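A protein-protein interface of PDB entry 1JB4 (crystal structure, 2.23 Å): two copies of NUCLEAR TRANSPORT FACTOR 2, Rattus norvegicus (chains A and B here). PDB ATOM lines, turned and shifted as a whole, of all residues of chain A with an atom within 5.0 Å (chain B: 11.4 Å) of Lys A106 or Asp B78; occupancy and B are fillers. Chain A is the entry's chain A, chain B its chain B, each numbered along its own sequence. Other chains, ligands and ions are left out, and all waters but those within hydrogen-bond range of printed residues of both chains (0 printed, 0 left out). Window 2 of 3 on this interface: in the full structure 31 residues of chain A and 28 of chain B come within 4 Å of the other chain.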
ATOM      1  N   ASP A  78     -21.149 -23.393  19.689  1.00  0.00           N
ATOM      2  CA  ASP A  78     -20.694 -22.065  19.294  1.00  0.00           C
ATOM      3  C   ASP A  78     -21.668 -21.290  18.397  1.00  0.00           C
ATOM      4  O   ASP A  78     -21.268 -20.335  17.720  1.00  0.00           O
ATOM      5  CB  ASP A  78     -19.329 -22.171  18.612  1.00  0.00           C
ATOM      6  CG  ASP A  78     -18.261 -22.719  19.547  1.00  0.00           C
ATOM      7  OD1 ASP A  78     -18.030 -22.084  20.599  1.00  0.00           O
ATOM      8  OD2 ASP A  78     -17.663 -23.777  19.246  1.00  0.00           O
ATOM      9  N   CYS A  80     -23.198 -22.297  15.629  1.00  0.00           N
ATOM     10  CA  CYS A  80     -23.113 -22.592  14.201  1.00  0.00           C
ATOM     11  C   CYS A  80     -24.223 -23.586  13.952  1.00  0.00           C
ATOM     12  O   CYS A  80     -24.856 -24.064  14.888  1.00  0.00           O
ATOM     13  CB  CYS A  80     -21.811 -23.288  13.812  1.00  0.00           C
ATOM     14  SG  CYS A  80     -20.323 -22.361  14.027  1.00  0.00           S
ATOM     15  N   LEU A 104     -21.216 -26.946   7.557  1.00  0.00           N
ATOM     16  CA  LEU A 104     -21.150 -26.357   8.883  1.00  0.00           C
ATOM     17  C   LEU A 104     -21.276 -24.882   8.515  1.00  0.00           C
ATOM     18  O   LEU A 104     -20.504 -24.361   7.705  1.00  0.00           O
ATOM     19  CB  LEU A 104     -19.829 -26.669   9.586  1.00  0.00           C
ATOM     20  CG  LEU A 104     -19.786 -26.092  11.005  1.00  0.00           C
ATOM     21  CD1 LEU A 104     -20.896 -26.749  11.838  1.00  0.00           C
ATOM     22  CD2 LEU A 104     -18.393 -26.298  11.644  1.00  0.00           C
ATOM     23  N   LEU A 105     -22.302 -24.231   9.047  1.00  0.00           N
ATOM     24  CA  LEU A 105     -22.544 -22.834   8.731  1.00  0.00           C
ATOM     25  C   LEU A 105     -22.262 -21.965   9.935  1.00  0.00           C
ATOM     26  O   LEU A 105     -22.384 -22.403  11.077  1.00  0.00           O
ATOM     27  CB  LEU A 105     -24.002 -22.643   8.282  1.00  0.00           C
ATOM     28  CG  LEU A 105     -24.530 -23.608   7.208  1.00  0.00           C
ATOM     29  CD1 LEU A 105     -26.003 -23.356   7.003  1.00  0.00           C
ATOM     30  CD2 LEU A 105     -23.761 -23.435   5.873  1.00  0.00           C
ATOM     31  N   LYS A 106     -21.876 -20.727   9.675  1.00  0.00           N
ATOM     32  CA  LYS A 106     -21.607 -19.795  10.744  1.00  0.00           C
ATOM     33  C   LYS A 106     -22.003 -18.402  10.284  1.00  0.00           C
ATOM     34  O   LYS A 106     -22.064 -18.120   9.087  1.00  0.00           O
ATOM     35  CB  LYS A 106     -20.121 -19.834  11.134  1.00  0.00           C
ATOM     36  CG  LYS A 106     -19.721 -18.779  12.172  1.00  0.00           C
ATOM     37  CD  LYS A 106     -18.505 -19.180  13.013  1.00  0.00           C
ATOM     38  CE  LYS A 106     -18.531 -18.419  14.353  1.00  0.00           C
ATOM     39  NZ  LYS A 106     -17.747 -19.066  15.431  1.00  0.00           N
ATOM     40  N   ASN A 107     -22.317 -17.546  11.247  1.00  0.00           N
ATOM     41  CA  ASN A 107     -22.665 -16.162  10.965  1.00  0.00           C
ATOM     42  C   ASN A 107     -21.350 -15.445  11.294  1.00  0.00           C
ATOM     43  O   ASN A 107     -20.895 -15.480  12.434  1.00  0.00           O
ATOM     44  CB  ASN A 107     -23.788 -15.695  11.899  1.00  0.00           C
ATOM     45  CG  ASN A 107     -24.294 -14.294  11.567  1.00  0.00           C
ATOM     46  OD1 ASN A 107     -25.388 -14.128  11.040  1.00  0.00           O
ATOM     47  ND2 ASN A 107     -23.497 -13.285  11.878  1.00  0.00           N
ATOM     48  N   ILE A 108     -20.740 -14.831  10.283  1.00  0.00           N
ATOM     49  CA  ILE A 108     -19.468 -14.120  10.423  1.00  0.00           C
ATOM     50  C   ILE A 108     -19.594 -12.753   9.760  1.00  0.00           C
ATOM     51  O   ILE A 108     -19.826 -12.676   8.550  1.00  0.00           O
ATOM     52  CB  ILE A 108     -18.314 -14.901   9.729  1.00  0.00           C
ATOM     53  CG1 ILE A 108     -18.004 -16.180  10.505  1.00  0.00           C
ATOM     54  CG2 ILE A 108     -17.061 -14.039   9.640  1.00  0.00           C
ATOM     55  CD1 ILE A 108     -16.883 -17.017   9.900  1.00  0.00           C
ATOM     56  N   ALA A 111     -23.456 -12.267   8.672  1.00  0.00           N
ATOM     57  CA  ALA A 111     -23.928 -12.887   7.434  1.00  0.00           C
ATOM     58  C   ALA A 111     -23.640 -14.378   7.532  1.00  0.00           C
ATOM     59  O   ALA A 111     -22.614 -14.776   8.083  1.00  0.00           O
ATOM     60  CB  ALA A 111     -23.209 -12.299   6.239  1.00  0.00           C
ATOM     61  N   TRP A 112     -24.533 -15.210   7.007  1.00  0.00           N
ATOM     62  CA  TRP A 112     -24.307 -16.644   7.077  1.00  0.00           C
ATOM     63  C   TRP A 112     -23.432 -17.160   5.945  1.00  0.00           C
ATOM     64  O   TRP A 112     -23.719 -16.943   4.773  1.00  0.00           O
ATOM     65  CB  TRP A 112     -25.633 -17.406   7.087  1.00  0.00           C
ATOM     66  CG  TRP A 112     -26.366 -17.291   8.386  1.00  0.00           C
ATOM     67  CD1 TRP A 112     -27.325 -16.376   8.706  1.00  0.00           C
ATOM     68  CD2 TRP A 112     -26.155 -18.082   9.564  1.00  0.00           C
ATOM     69  NE1 TRP A 112     -27.722 -16.545  10.005  1.00  0.00           N
ATOM     70  CE2 TRP A 112     -27.021 -17.584  10.557  1.00  0.00           C
ATOM     71  CE3 TRP A 112     -25.315 -19.160   9.876  1.00  0.00           C
ATOM     72  CZ2 TRP A 112     -27.077 -18.125  11.848  1.00  0.00           C
ATOM     73  CZ3 TRP A 112     -25.367 -19.701  11.162  1.00  0.00           C
ATOM     74  CH2 TRP A 112     -26.246 -19.179  12.132  1.00  0.00           C
ATOM     75  N   VAL A 113     -22.353 -17.841   6.317  1.00  0.00           N
ATOM     76  CA  VAL A 113     -21.437 -18.413   5.350  1.00  0.00           C
ATOM     77  C   VAL A 113     -21.189 -19.874   5.689  1.00  0.00           C
ATOM     78  O   VAL A 113     -21.476 -20.329   6.793  1.00  0.00           O
ATOM     79  CB  VAL A 113     -20.084 -17.675   5.346  1.00  0.00           C
ATOM     80  CG1 VAL A 113     -20.294 -16.204   5.057  1.00  0.00           C
ATOM     81  CG2 VAL A 113     -19.374 -17.876   6.677  1.00  0.00           C
ATOM     82  N   THR A 115     -18.421 -22.624   6.299  1.00  0.00           N
ATOM     83  CA  THR A 115     -16.989 -22.714   6.547  1.00  0.00           C
ATOM     84  C   THR A 115     -16.458 -24.110   6.236  1.00  0.00           C
ATOM     85  O   THR A 115     -15.254 -24.302   6.030  1.00  0.00           O
ATOM     86  CB  THR A 115     -16.631 -22.345   8.012  1.00  0.00           C
ATOM     87  OG1 THR A 115     -17.041 -23.396   8.891  1.00  0.00           O
ATOM     88  CG2 THR A 115     -17.312 -21.042   8.418  1.00  0.00           C
ATOM     89  N   ILE B   6      -3.165 -32.423  11.692  1.00  0.00           N
ATOM     90  CA  ILE B   6      -3.620 -32.645  13.056  1.00  0.00           C
ATOM     91  C   ILE B   6      -5.136 -32.885  13.212  1.00  0.00           C
ATOM     92  O   ILE B   6      -5.541 -33.710  14.027  1.00  0.00           O
ATOM     93  CB  ILE B   6      -3.152 -31.472  13.976  1.00  0.00           C
ATOM     94  CG1 ILE B   6      -2.391 -32.032  15.183  1.00  0.00           C
ATOM     95  CG2 ILE B   6      -4.323 -30.623  14.409  1.00  0.00           C
ATOM     96  CD1 ILE B   6      -3.115 -33.140  15.922  1.00  0.00           C
ATOM     97  N   TRP B   7      -5.974 -32.187  12.445  1.00  0.00           N
ATOM     98  CA  TRP B   7      -7.419 -32.396  12.565  1.00  0.00           C
ATOM     99  C   TRP B   7      -7.782 -33.801  12.082  1.00  0.00           C
ATOM    100  O   TRP B   7      -8.653 -34.465  12.656  1.00  0.00           O
ATOM    101  CB  TRP B   7      -8.203 -31.326  11.786  1.00  0.00           C
ATOM    102  CG  TRP B   7      -7.824 -31.203  10.343  1.00  0.00           C
ATOM    103  CD1 TRP B   7      -8.264 -31.979   9.310  1.00  0.00           C
ATOM    104  CD2 TRP B   7      -6.898 -30.263   9.778  1.00  0.00           C
ATOM    105  NE1 TRP B   7      -7.671 -31.582   8.132  1.00  0.00           N
ATOM    106  CE2 TRP B   7      -6.828 -30.530   8.389  1.00  0.00           C
ATOM    107  CE3 TRP B   7      -6.119 -29.219  10.310  1.00  0.00           C
ATOM    108  CZ2 TRP B   7      -6.004 -29.791   7.516  1.00  0.00           C
ATOM    109  CZ3 TRP B   7      -5.295 -28.483   9.438  1.00  0.00           C
ATOM    110  CH2 TRP B   7      -5.249 -28.778   8.056  1.00  0.00           C
ATOM    111  N   GLN B  74     -11.969 -32.086   8.617  1.00  0.00           N
ATOM    112  CA  GLN B  74     -11.550 -30.709   8.353  1.00  0.00           C
ATOM    113  C   GLN B  74     -11.543 -29.897   9.644  1.00  0.00           C
ATOM    114  O   GLN B  74     -12.279 -30.196  10.587  1.00  0.00           O
ATOM    115  CB  GLN B  74     -12.498 -30.006   7.378  1.00  0.00           C
ATOM    116  CG  GLN B  74     -12.692 -30.647   6.012  1.00  0.00           C
ATOM    117  CD  GLN B  74     -13.777 -29.928   5.219  1.00  0.00           C
ATOM    118  OE1 GLN B  74     -14.576 -29.171   5.787  1.00  0.00           O
ATOM    119  NE2 GLN B  74     -13.822 -30.166   3.911  1.00  0.00           N
ATOM    120  N   PRO B  75     -10.691 -28.866   9.715  1.00  0.00           N
ATOM    121  CA  PRO B  75     -10.674 -28.057  10.932  1.00  0.00           C
ATOM    122  C   PRO B  75     -11.723 -26.964  10.725  1.00  0.00           C
ATOM    123  O   PRO B  75     -12.046 -26.617   9.577  1.00  0.00           O
ATOM    124  CB  PRO B  75      -9.258 -27.488  10.940  1.00  0.00           C
ATOM    125  CG  PRO B  75      -9.006 -27.256   9.473  1.00  0.00           C
ATOM    126  CD  PRO B  75      -9.548 -28.532   8.840  1.00  0.00           C
ATOM    127  N   THR B  76     -12.267 -26.437  11.813  1.00  0.00           N
ATOM    128  CA  THR B  76     -13.248 -25.357  11.704  1.00  0.00           C
ATOM    129  C   THR B  76     -12.646 -24.099  12.331  1.00  0.00           C
ATOM    130  O   THR B  76     -11.688 -24.177  13.096  1.00  0.00           O
ATOM    131  CB  THR B  76     -14.583 -25.703  12.419  1.00  0.00           C
ATOM    132  OG1 THR B  76     -14.420 -25.612  13.841  1.00  0.00           O
ATOM    133  CG2 THR B  76     -15.020 -27.110  12.044  1.00  0.00           C
ATOM    134  N   PRO B  77     -13.194 -22.922  12.006  1.00  0.00           N
ATOM    135  CA  PRO B  77     -12.681 -21.660  12.554  1.00  0.00           C
ATOM    136  C   PRO B  77     -12.645 -21.572  14.092  1.00  0.00           C
ATOM    137  O   PRO B  77     -11.803 -20.862  14.655  1.00  0.00           O
ATOM    138  CB  PRO B  77     -13.604 -20.614  11.923  1.00  0.00           C
ATOM    139  CG  PRO B  77     -13.982 -21.261  10.599  1.00  0.00           C
ATOM    140  CD  PRO B  77     -14.280 -22.673  11.041  1.00  0.00           C
ATOM    141  N   ASP B  78     -13.547 -22.282  14.767  1.00  0.00           N
ATOM    142  CA  ASP B  78     -13.588 -22.266  16.227  1.00  0.00           C
ATOM    143  C   ASP B  78     -12.746 -23.394  16.822  1.00  0.00           C
ATOM    144  O   ASP B  78     -12.931 -23.766  17.979  1.00  0.00           O
ATOM    145  CB  ASP B  78     -15.034 -22.390  16.731  1.00  0.00           C
ATOM    146  CG  ASP B  78     -15.932 -21.274  16.221  1.00  0.00           C
ATOM    147  OD1 ASP B  78     -15.600 -20.090  16.439  1.00  0.00           O
ATOM    148  OD2 ASP B  78     -16.975 -21.580  15.602  1.00  0.00           O
ATOM    149  N   SER B  79     -11.833 -23.940  16.025  1.00  0.00           N
ATOM    150  CA  SER B  79     -10.961 -25.014  16.481  1.00  0.00           C
ATOM    151  C   SER B  79     -11.690 -26.330  16.731  1.00  0.00           C
ATOM    152  O   SER B  79     -11.244 -27.164  17.523  1.00  0.00           O
ATOM    153  CB  SER B  79     -10.225 -24.590  17.753  1.00  0.00           C
ATOM    154  OG  SER B  79      -9.540 -23.374  17.535  1.00  0.00           O
ATOM    155  N   CYS B  80     -12.830 -26.503  16.078  1.00  0.00           N
ATOM    156  CA  CYS B  80     -13.570 -27.747  16.198  1.00  0.00           C
ATOM    157  C   CYS B  80     -13.096 -28.551  15.005  1.00  0.00           C
ATOM    158  O   CYS B  80     -12.417 -28.016  14.128  1.00  0.00           O
ATOM    159  CB  CYS B  80     -15.082 -27.519  16.078  1.00  0.00           C
ATOM    160  SG  CYS B  80     -15.840 -26.656  17.481  1.00  0.00           S
ATOM    161  N   ILE B  81     -13.431 -29.836  14.984  1.00  0.00           N
ATOM    162  CA  ILE B  81     -13.068 -30.688  13.866  1.00  0.00           C
ATOM    163  C   ILE B  81     -14.363 -31.285  13.355  1.00  0.00           C
ATOM    164  O   ILE B  81     -15.125 -31.865  14.126  1.00  0.00           O
ATOM    165  CB  ILE B  81     -12.129 -31.843  14.289  1.00  0.00           C
ATOM    166  CG1 ILE B  81     -10.741 -31.306  14.652  1.00  0.00           C
ATOM    167  CG2 ILE B  81     -11.958 -32.819  13.126  1.00  0.00           C
ATOM    168  CD1 ILE B  81     -10.756 -30.123  15.580  1.00  0.00           C
ATOM    169  N   ILE B  82     -14.634 -31.131  12.066  1.00  0.00           N
ATOM    170  CA  ILE B  82     -15.853 -31.713  11.518  1.00  0.00           C
ATOM    171  C   ILE B  82     -15.488 -32.931  10.679  1.00  0.00           C
ATOM    172  O   ILE B  82     -14.527 -32.894   9.907  1.00  0.00           O
ATOM    173  CB  ILE B  82     -16.646 -30.715  10.656  1.00  0.00           C
ATOM    174  CG1 ILE B  82     -17.972 -31.370  10.259  1.00  0.00           C
ATOM    175  CG2 ILE B  82     -15.825 -30.276   9.433  1.00  0.00           C
ATOM    176  CD1 ILE B  82     -18.919 -30.469   9.516  1.00  0.00           C
ATOM    177  N   LEU B 104     -19.160 -33.606  14.842  1.00  0.00           N
ATOM    178  CA  LEU B 104     -18.540 -32.313  15.037  1.00  0.00           C
ATOM    179  C   LEU B 104     -17.836 -32.514  16.371  1.00  0.00           C
ATOM    180  O   LEU B 104     -18.468 -32.888  17.356  1.00  0.00           O
ATOM    181  CB  LEU B 104     -19.578 -31.201  15.138  1.00  0.00           C
ATOM    182  CG  LEU B 104     -18.940 -29.812  15.257  1.00  0.00           C
ATOM    183  CD1 LEU B 104     -18.029 -29.568  14.049  1.00  0.00           C
ATOM    184  CD2 LEU B 104     -20.016 -28.736  15.362  1.00  0.00           C
ATOM    185  N   LEU B 105     -16.524 -32.312  16.401  1.00  0.00           N
ATOM    186  CA  LEU B 105     -15.770 -32.495  17.639  1.00  0.00           C
ATOM    187  C   LEU B 105     -15.180 -31.194  18.160  1.00  0.00           C
ATOM    188  O   LEU B 105     -14.929 -30.265  17.393  1.00  0.00           O
ATOM    189  CB  LEU B 105     -14.633 -33.489  17.419  1.00  0.00           C
ATOM    190  CG  LEU B 105     -14.923 -34.717  16.557  1.00  0.00           C
ATOM    191  CD1 LEU B 105     -13.638 -35.529  16.371  1.00  0.00           C
ATOM    192  CD2 LEU B 105     -16.017 -35.550  17.188  1.00  0.00           C
ATOM    193  N   LYS B 106     -14.948 -31.136  19.469  1.00  0.00           N
ATOM    194  CA  LYS B 106     -14.365 -29.952  20.096  1.00  0.00           C
ATOM    195  C   LYS B 106     -13.686 -30.384  21.387  1.00  0.00           C
ATOM    196  O   LYS B 106     -14.089 -31.367  22.000  1.00  0.00           O
ATOM    197  CB  LYS B 106     -15.445 -28.909  20.409  1.00  0.00           C
ATOM    198  CG  LYS B 106     -14.881 -27.576  20.889  1.00  0.00           C
ATOM    199  CD  LYS B 106     -15.959 -26.532  21.150  1.00  0.00           C
ATOM    200  CE  LYS B 106     -15.334 -25.143  21.275  1.00  0.00           C
ATOM    201  NZ  LYS B 106     -16.299 -24.076  21.634  1.00  0.00           N
ATOM    202  N   ASN B 107     -12.646 -29.663  21.788  1.00  0.00           N
ATOM    203  CA  ASN B 107     -11.941 -29.983  23.020  1.00  0.00           C
ATOM    204  C   ASN B 107     -12.573 -29.201  24.167  1.00  0.00           C
ATOM    205  O   ASN B 107     -12.471 -27.977  24.224  1.00  0.00           O
ATOM    206  CB  ASN B 107     -10.468 -29.619  22.911  1.00  0.00           C
ATOM    207  CG  ASN B 107      -9.678 -30.046  24.136  1.00  0.00           C
ATOM    208  OD1 ASN B 107      -9.222 -31.189  24.232  1.00  0.00           O
ATOM    209  ND2 ASN B 107      -9.535 -29.136  25.093  1.00  0.00           N
ATOM    210  N   ILE B 108     -13.225 -29.916  25.075  1.00  0.00           N
ATOM    211  CA  ILE B 108     -13.900 -29.305  26.218  1.00  0.00           C
ATOM    212  C   ILE B 108     -13.426 -29.933  27.526  1.00  0.00           C
ATOM    213  O   ILE B 108     -13.439 -31.163  27.683  1.00  0.00           O
ATOM    214  CB  ILE B 108     -15.436 -29.473  26.104  1.00  0.00           C
ATOM    215  CG1 ILE B 108     -15.949 -28.697  24.886  1.00  0.00           C
ATOM    216  CG2 ILE B 108     -16.124 -28.971  27.372  1.00  0.00           C
ATOM    217  CD1 ILE B 108     -17.393 -28.993  24.540  1.00  0.00           C
ATOM    218  N   ALA B 111     -10.884 -32.618  26.894  1.00  0.00           N
ATOM    219  CA  ALA B 111     -11.241 -33.852  26.200  1.00  0.00           C
ATOM    220  C   ALA B 111     -11.974 -33.575  24.902  1.00  0.00           C
ATOM    221  O   ALA B 111     -12.798 -32.665  24.835  1.00  0.00           O
ATOM    222  CB  ALA B 111     -12.109 -34.734  27.105  1.00  0.00           C
ATOM    223  N   TRP B 112     -11.663 -34.353  23.869  1.00  0.00           N
ATOM    224  CA  TRP B 112     -12.343 -34.190  22.597  1.00  0.00           C
ATOM    225  C   TRP B 112     -13.686 -34.904  22.677  1.00  0.00           C
ATOM    226  O   TRP B 112     -13.747 -36.126  22.797  1.00  0.00           O
ATOM    227  CB  TRP B 112     -11.517 -34.770  21.453  1.00  0.00           C
ATOM    228  CG  TRP B 112     -10.434 -33.850  21.005  1.00  0.00           C
ATOM    229  CD1 TRP B 112      -9.130 -33.855  21.413  1.00  0.00           C
ATOM    230  CD2 TRP B 112     -10.577 -32.733  20.121  1.00  0.00           C
ATOM    231  NE1 TRP B 112      -8.456 -32.804  20.842  1.00  0.00           N
ATOM    232  CE2 TRP B 112      -9.318 -32.100  20.044  1.00  0.00           C
ATOM    233  CE3 TRP B 112     -11.647 -32.202  19.389  1.00  0.00           C
ATOM    234  CZ2 TRP B 112      -9.098 -30.961  19.261  1.00  0.00           C
ATOM    235  CZ3 TRP B 112     -11.430 -31.067  18.609  1.00  0.00           C
ATOM    236  CH2 TRP B 112     -10.163 -30.461  18.554  1.00  0.00           C
ATOM    237  N   VAL B 113     -14.763 -34.131  22.642  1.00  0.00           N
ATOM    238  CA  VAL B 113     -16.091 -34.715  22.705  1.00  0.00           C
ATOM    239  C   VAL B 113     -16.869 -34.355  21.449  1.00  0.00           C
ATOM    240  O   VAL B 113     -16.508 -33.420  20.703  1.00  0.00           O
ATOM    241  CB  VAL B 113     -16.888 -34.214  23.945  1.00  0.00           C
ATOM    242  CG1 VAL B 113     -16.175 -34.602  25.223  1.00  0.00           C
ATOM    243  CG2 VAL B 113     -17.065 -32.701  23.875  1.00  0.00           C
ATOM    244  N   THR B 115     -20.108 -32.855  19.935  1.00  0.00           N
ATOM    245  CA  THR B 115     -21.234 -31.987  20.252  1.00  0.00           C
ATOM    246  C   THR B 115     -22.383 -32.231  19.267  1.00  0.00           C
ATOM    247  O   THR B 115     -23.549 -31.985  19.585  1.00  0.00           O
ATOM    248  CB  THR B 115     -20.851 -30.495  20.180  1.00  0.00           C
ATOM    249  OG1 THR B 115     -20.380 -30.185  18.864  1.00  0.00           O
ATOM    250  CG2 THR B 115     -19.776 -30.161  21.204  1.00  0.00           C
ATOM    251  N   ASN B 116     -22.046 -32.733  18.082  1.00  0.00           N
ATOM    252  CA  ASN B 116     -23.035 -32.966  17.049  1.00  0.00           C
ATOM    253  C   ASN B 116     -22.800 -34.275  16.331  1.00  0.00           C
ATOM    254  O   ASN B 116     -21.706 -34.535  15.821  1.00  0.00           O
ATOM    255  CB  ASN B 116     -23.012 -31.791  16.069  1.00  0.00           C
ATOM    256  CG  ASN B 116     -23.390 -30.474  16.737  1.00  0.00           C
ATOM    257  OD1 ASN B 116     -24.564 -30.115  16.805  1.00  0.00           O
ATOM    258  ND2 ASN B 116     -22.394 -29.763  17.255  1.00  0.00           N
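Asp A78 touches just these residues of chain B: Asp B78, Cys B80 and Lys B106. Of chain B, only Asp B78 comes within 4 Å of Cys A80. Of chain B, only Thr B76 and Ile B82 come within 4 Å of Leu A104. Lys A106 touches just one residue of chain B: Asp B78. No residue of chain B comes within 4 Å of Asn A107. Ala A111 touches none of the printed residues of chain B. No residue of chain B comes within 4 Å of Trp A112. Printed residues of chain A within 4 Å of Thr B76: Leu A104 (3.5 Å). Of the printed residues of chain A, Pro B77 touches Thr A115 (3.6 Å). Asp B78 touches three residues of chain A. Of the printed residues of chain A, Cys B80 touches Asp A78 (3.8 Å). Of the printed residues of chain A, Ile B82 touches Leu A104. Leu B104 touches none of the printed residues of chain A. Of the printed residues of chain A, Lys B106 touches Asp A78. The nearest residue of chain B that does not touch Lys A106 is Pro B77 (5.2 Å). The nearest printed residue of chain A that does not touch Asp B78 is Leu A104 (6.3 Å).
Among the printed residues, merely in contact across the chains: Asp A78 with Asp B78, Asp A78 with Cys B80, Leu A104 with Thr B76, Leu A104 with Ile B82 and Thr A115 with Pro B77.
Hydrophobic or aromatic side chains of chain A that line the printed part of chain B: Leu A104. Of the 21 printed residues of chain B, 6 touch a printed residue of chain A. Printed residues of chain B that touch a printed residue of chain A: Thr B76, Pro B77, Asp B78, Cys B80, Ile B82 and Lys B106. Among the printed residues, 8 pairs touch across the chains. Among the printed residues, Asp or Glu carboxylates within 4 Å of a Lys or Arg side-chain nitrogen of the other chain: Asp A78 with Lys B106 and Lys A106 with Asp B78.
Asp B78 touches its own counterpart, Asp A78. Asp A78 touches Cys B80, and with the chains exchanged Cys A80 touches Asp B78. Asp A78 touches Lys B106, and with the chains exchanged Lys A106 touches Asp B78.
The side-chain carboxylate (OD2) of Asp A78 is in salt-bridge range of the side-chain amino group (NZ) of Lys B106, 2.8 Å away. SG of Cys A80 sits at hydrogen-bond distance from OD2 of Asp B78 (3.8 Å). NZ of Lys A106 is in salt-bridge range of OD1 of Asp B78 (2.6 Å).
O of Leu A104 lies within hydrogen-bond range of N of Thr A115, at 3.1 Å. The backbone NH of Val A113 sits at hydrogen-bond distance from the backbone carbonyl oxygen of Lys A106. The backbone carbonyl oxygen (O) of Gln B74 is in hydrogen-bond range of the backbone NH (N) of Ile B82 (2.9 Å). OG1 of Thr B76 lies within hydrogen-bond range of N of Cys B80 (2.9 Å). The side-chain sulfur of Cys B80 lies close to the backbone carbonyl oxygen of Leu B105 (3.7 Å). The backbone carbonyl oxygen of Lys B106 lies within hydrogen-bond range of the backbone NH of Val B113.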
